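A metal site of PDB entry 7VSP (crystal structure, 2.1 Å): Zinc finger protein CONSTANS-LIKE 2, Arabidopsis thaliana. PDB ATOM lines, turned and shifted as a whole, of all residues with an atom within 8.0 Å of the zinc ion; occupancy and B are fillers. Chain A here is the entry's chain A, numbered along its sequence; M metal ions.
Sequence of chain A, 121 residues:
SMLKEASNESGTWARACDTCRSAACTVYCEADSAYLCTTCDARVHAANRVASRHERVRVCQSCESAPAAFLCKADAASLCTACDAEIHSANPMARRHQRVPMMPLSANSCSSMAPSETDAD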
ATOM      1  N   ALA A  16      -5.696  23.100   4.328  1.00  0.00           N
ATOM      2  CA  ALA A  16      -6.968  22.509   3.901  1.00  0.00           C
ATOM      3  C   ALA A  16      -8.111  22.652   4.921  1.00  0.00           C
ATOM      4  O   ALA A  16      -7.910  22.664   6.141  1.00  0.00           O
ATOM      5  CB  ALA A  16      -6.790  21.020   3.609  1.00  0.00           C
ATOM      6  N   CYS A  17      -9.332  22.686   4.417  1.00  0.00           N
ATOM      7  CA  CYS A  17     -10.511  22.626   5.269  1.00  0.00           C
ATOM      8  C   CYS A  17     -10.478  21.342   6.088  1.00  0.00           C
ATOM      9  O   CYS A  17     -10.188  20.274   5.546  1.00  0.00           O
ATOM     10  CB  CYS A  17     -11.770  22.693   4.420  1.00  0.00           C
ATOM     11  SG  CYS A  17     -13.308  22.548   5.351  1.00  0.00           S
ATOM     12  N   ASP A  18     -10.749  21.456   7.413  1.00  0.00           N
ATOM     13  CA  ASP A  18     -10.700  20.269   8.272  1.00  0.00           C
ATOM     14  C   ASP A  18     -11.864  19.315   8.034  1.00  0.00           C
ATOM     15  O   ASP A  18     -11.742  18.127   8.354  1.00  0.00           O
ATOM     16  CB  ASP A  18     -10.718  20.638   9.769  1.00  0.00           C
ATOM     17  CG  ASP A  18      -9.393  21.180  10.269  1.00  0.00           C
ATOM     18  OD1 ASP A  18      -8.319  20.748   9.796  1.00  0.00           O
ATOM     19  OD2 ASP A  18      -9.439  22.092  11.138  1.00  0.00           O
ATOM     20  N   THR A  19     -12.991  19.780   7.500  1.00  0.00           N
ATOM     21  CA  THR A  19     -14.104  18.856   7.273  1.00  0.00           C
ATOM     22  C   THR A  19     -14.098  18.269   5.859  1.00  0.00           C
ATOM     23  O   THR A  19     -14.137  17.042   5.698  1.00  0.00           O
ATOM     24  CB  THR A  19     -15.443  19.535   7.538  1.00  0.00           C
ATOM     25  OG1 THR A  19     -15.518  20.776   6.849  1.00  0.00           O
ATOM     26  CG2 THR A  19     -15.582  19.806   8.995  1.00  0.00           C
ATOM     27  N   CYS A  20     -14.061  19.095   4.824  1.00  0.00           N
ATOM     28  CA  CYS A  20     -14.120  18.550   3.473  1.00  0.00           C
ATOM     29  C   CYS A  20     -12.760  18.190   2.928  1.00  0.00           C
ATOM     30  O   CYS A  20     -12.678  17.312   2.053  1.00  0.00           O
ATOM     31  CB  CYS A  20     -14.813  19.526   2.520  1.00  0.00           C
ATOM     32  SG  CYS A  20     -13.825  20.925   1.882  1.00  0.00           S
ATOM     33  N   ARG A  21     -11.714  18.856   3.408  1.00  0.00           N
ATOM     34  CA  ARG A  21     -10.320  18.484   3.020  1.00  0.00           C
ATOM     35  C   ARG A  21     -10.176  18.519   1.500  1.00  0.00           C
ATOM     36  O   ARG A  21      -9.348  17.760   0.967  1.00  0.00           O
ATOM     37  CB  ARG A  21      -9.968  17.102   3.579  1.00  0.00           C
ATOM     38  CG  ARG A  21      -9.623  17.094   5.066  1.00  0.00           C
ATOM     39  CD  ARG A  21      -8.316  16.389   5.353  1.00  0.00           C
ATOM     40  NE  ARG A  21      -8.299  15.031   4.830  1.00  0.00           N
ATOM     41  CZ  ARG A  21      -8.164  13.939   5.575  1.00  0.00           C
ATOM     42  NH1 ARG A  21      -8.034  14.038   6.883  1.00  0.00           N
ATOM     43  NH2 ARG A  21      -8.150  12.746   5.000  1.00  0.00           N
ATOM     44  N   SER A  22     -10.957  19.369   0.839  1.00  0.00           N
ATOM     45  CA  SER A  22     -10.853  19.518  -0.609  1.00  0.00           C
ATOM     46  C   SER A  22     -10.870  20.973  -1.034  1.00  0.00           C
ATOM     47  O   SER A  22     -10.893  21.255  -2.233  1.00  0.00           O
ATOM     48  CB  SER A  22     -12.002  18.786  -1.297  1.00  0.00           C
ATOM     49  OG  SER A  22     -12.294  17.561  -0.645  1.00  0.00           O
ATOM     50  N   ALA A  23     -10.866  21.900  -0.093  1.00  0.00           N
ATOM     51  CA  ALA A  23     -10.842  23.312  -0.388  1.00  0.00           C
ATOM     52  C   ALA A  23      -9.932  23.986   0.617  1.00  0.00           C
ATOM     53  O   ALA A  23      -9.695  23.451   1.708  1.00  0.00           O
ATOM     54  CB  ALA A  23     -12.244  23.911  -0.338  1.00  0.00           C
ATOM     55  N   ALA A  24      -9.414  25.150   0.255  1.00  0.00           N
ATOM     56  CA  ALA A  24      -8.654  25.946   1.204  1.00  0.00           C
ATOM     57  C   ALA A  24      -9.574  26.434   2.319  1.00  0.00           C
ATOM     58  O   ALA A  24     -10.713  26.850   2.059  1.00  0.00           O
ATOM     59  CB  ALA A  24      -7.995  27.114   0.478  1.00  0.00           C
ATOM     60  N   CYS A  25      -9.085  26.378   3.558  1.00  0.00           N
ATOM     61  CA  CYS A  25      -9.821  26.986   4.666  1.00  0.00           C
ATOM     62  C   CYS A  25      -9.889  28.494   4.471  1.00  0.00           C
ATOM     63  O   CYS A  25      -8.979  29.121   3.934  1.00  0.00           O
ATOM     64  CB  CYS A  25      -9.164  26.643   6.007  1.00  0.00           C
ATOM     65  SG  CYS A  25      -7.511  27.442   6.307  1.00  0.00           S
ATOM     66  N   THR A  26     -11.007  29.090   4.882  1.00  0.00           N
ATOM     67  CA  THR A  26     -11.115  30.543   4.836  1.00  0.00           C
ATOM     68  C   THR A  26     -11.444  31.164   6.179  1.00  0.00           C
ATOM     69  O   THR A  26     -11.208  32.366   6.365  1.00  0.00           O
ATOM     70  CB  THR A  26     -12.198  30.957   3.833  1.00  0.00           C
ATOM     71  OG1 THR A  26     -13.432  30.347   4.208  1.00  0.00           O
ATOM     72  CG2 THR A  26     -11.801  30.509   2.380  1.00  0.00           C
ATOM     73  N   TYR A  35     -10.415  24.729  11.144  1.00  0.00           N
ATOM     74  CA  TYR A  35     -10.257  25.523   9.937  1.00  0.00           C
ATOM     75  C   TYR A  35     -11.251  25.030   8.894  1.00  0.00           C
ATOM     76  O   TYR A  35     -11.302  23.838   8.596  1.00  0.00           O
ATOM     77  CB  TYR A  35      -8.831  25.404   9.391  1.00  0.00           C
ATOM     78  CG  TYR A  35      -7.809  25.987  10.341  1.00  0.00           C
ATOM     79  CD1 TYR A  35      -7.215  25.222  11.336  1.00  0.00           C
ATOM     80  CD2 TYR A  35      -7.408  27.304  10.208  1.00  0.00           C
ATOM     81  CE1 TYR A  35      -6.249  25.765  12.189  1.00  0.00           C
ATOM     82  CE2 TYR A  35      -6.463  27.852  11.039  1.00  0.00           C
ATOM     83  CZ  TYR A  35      -5.895  27.085  12.018  1.00  0.00           C
ATOM     84  OH  TYR A  35      -4.969  27.686  12.815  1.00  0.00           O
ATOM     85  N   LEU A  36     -12.018  25.948   8.335  1.00  0.00           N
ATOM     86  CA  LEU A  36     -13.105  25.562   7.431  1.00  0.00           C
ATOM     87  C   LEU A  36     -13.124  26.445   6.196  1.00  0.00           C
ATOM     88  O   LEU A  36     -12.893  27.651   6.295  1.00  0.00           O
ATOM     89  CB  LEU A  36     -14.478  25.675   8.120  1.00  0.00           C
ATOM     90  CG  LEU A  36     -14.585  24.856   9.420  1.00  0.00           C
ATOM     91  CD1 LEU A  36     -15.806  25.232  10.234  1.00  0.00           C
ATOM     92  CD2 LEU A  36     -14.578  23.356   9.100  1.00  0.00           C
ATOM     93  N   CYS A  37     -13.482  25.852   5.066  1.00  0.00           N
ATOM     94  CA  CYS A  37     -13.757  26.602   3.861  1.00  0.00           C
ATOM     95  C   CYS A  37     -15.099  27.276   4.016  1.00  0.00           C
ATOM     96  O   CYS A  37     -15.815  27.030   4.977  1.00  0.00           O
ATOM     97  CB  CYS A  37     -13.767  25.693   2.623  1.00  0.00           C
ATOM     98  SG  CYS A  37     -15.176  24.482   2.585  1.00  0.00           S
ATOM     99  N   THR A  38     -15.491  28.109   3.048  1.00  0.00           N
ATOM    100  CA  THR A  38     -16.696  28.893   3.293  1.00  0.00           C
ATOM    101  C   THR A  38     -17.956  28.026   3.336  1.00  0.00           C
ATOM    102  O   THR A  38     -18.824  28.223   4.189  1.00  0.00           O
ATOM    103  CB  THR A  38     -16.805  30.003   2.254  1.00  0.00           C
ATOM    104  OG1 THR A  38     -15.703  30.893   2.427  1.00  0.00           O
ATOM    105  CG2 THR A  38     -18.134  30.771   2.415  1.00  0.00           C
ATOM    106  N   THR A  39     -18.072  27.046   2.432  1.00  0.00           N
ATOM    107  CA  THR A  39     -19.305  26.269   2.458  1.00  0.00           C
ATOM    108  C   THR A  39     -19.367  25.386   3.693  1.00  0.00           C
ATOM    109  O   THR A  39     -20.443  25.264   4.307  1.00  0.00           O
ATOM    110  CB  THR A  39     -19.456  25.468   1.170  1.00  0.00           C
ATOM    111  OG1 THR A  39     -18.742  24.230   1.278  1.00  0.00           O
ATOM    112  CG2 THR A  39     -18.961  26.251  -0.010  1.00  0.00           C
ATOM    113  N   CYS A  40     -18.256  24.781   4.115  1.00  0.00           N
ATOM    114  CA  CYS A  40     -18.307  23.959   5.325  1.00  0.00           C
ATOM    115  C   CYS A  40     -18.609  24.810   6.560  1.00  0.00           C
ATOM    116  O   CYS A  40     -19.354  24.372   7.456  1.00  0.00           O
ATOM    117  CB  CYS A  40     -16.987  23.191   5.484  1.00  0.00           C
ATOM    118  SG  CYS A  40     -16.818  21.770   4.319  1.00  0.00           S
ATOM    119  N   ASP A  41     -18.070  26.027   6.615  1.00  0.00           N
ATOM    120  CA  ASP A  41     -18.401  26.927   7.702  1.00  0.00           C
ATOM    121  C   ASP A  41     -19.904  27.180   7.784  1.00  0.00           C
ATOM    122  O   ASP A  41     -20.491  27.184   8.890  1.00  0.00           O
ATOM    123  CB  ASP A  41     -17.651  28.239   7.519  1.00  0.00           C
ATOM    124  CG  ASP A  41     -17.965  29.238   8.605  1.00  0.00           C
ATOM    125  OD1 ASP A  41     -17.612  28.990   9.779  1.00  0.00           O
ATOM    126  OD2 ASP A  41     -18.573  30.278   8.308  1.00  0.00           O
ATOM    127  N   ARG A  43     -22.319  25.202   6.600  1.00  0.00           N
ATOM    128  CA  ARG A  43     -23.042  23.979   6.958  1.00  0.00           C
ATOM    129  C   ARG A  43     -22.896  23.641   8.423  1.00  0.00           C
ATOM    130  O   ARG A  43     -23.799  23.056   9.019  1.00  0.00           O
ATOM    131  CB  ARG A  43     -22.564  22.783   6.145  1.00  0.00           C
ATOM    132  CG  ARG A  43     -22.938  22.783   4.649  1.00  0.00           C
ATOM    133  CD  ARG A  43     -21.734  22.364   3.829  1.00  0.00           C
ATOM    134  NE  ARG A  43     -22.014  21.479   2.703  1.00  0.00           N
ATOM    135  CZ  ARG A  43     -21.086  20.908   1.929  1.00  0.00           C
ATOM    136  NH1 ARG A  43     -19.787  21.080   2.168  1.00  0.00           N
ATOM    137  NH2 ARG A  43     -21.471  20.169   0.898  1.00  0.00           N
ATOM    138  N   VAL A  44     -21.723  23.935   9.005  1.00  0.00           N
ATOM    139  CA  VAL A  44     -21.492  23.588  10.390  1.00  0.00           C
ATOM    140  C   VAL A  44     -22.308  24.496  11.307  1.00  0.00           C
ATOM    141  O   VAL A  44     -22.904  24.046  12.289  1.00  0.00           O
ATOM    142  CB  VAL A  44     -19.983  23.643  10.722  1.00  0.00           C
ATOM    143  CG1 VAL A  44     -19.760  23.651  12.232  1.00  0.00           C
ATOM    144  CG2 VAL A  44     -19.215  22.440  10.032  1.00  0.00           C
HETATM  145 ZN    ZN M   1     -14.726  22.437   3.518  1.00  0.00          ZN
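The side-chain hydroxyl (OG) of Ser 22 sits at hydrogen-bond distance from the backbone carbonyl oxygen (O) of Cys 20, 2.7 Å away.
SG of Cys 40 sits close to OG1 of Thr 19 (3.0 Å).
O of Ala 23 sits at hydrogen-bond distance from N of Cys 17, 2.8 Å away.
The side-chain sulfur (SG) of Cys 40 sits close to the guanidinium group (NH1) of Arg 43 (3.7 Å).
The side-chain sulfur (SG) of Cys 17 lies close to the side-chain hydroxyl (OG1) of Thr 19 (3.2 Å).
The side-chain sulfur of Cys 20 sits close to the backbone NH of Ala 23 (3.7 Å).
Merely in contact with the zinc ion: Thr 19 (3.8 Å).
Within 4 Å of the zinc ion: Cys 17, Thr 19, Cys 20, Cys 37 and Cys 40.
The zinc ion is bound by SG of Cys 37 (2.3 Å), SG of Cys 17 (2.3 Å), SG of Cys 40 (2.3 Å) and SG of Cys 20 (2.4 Å).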
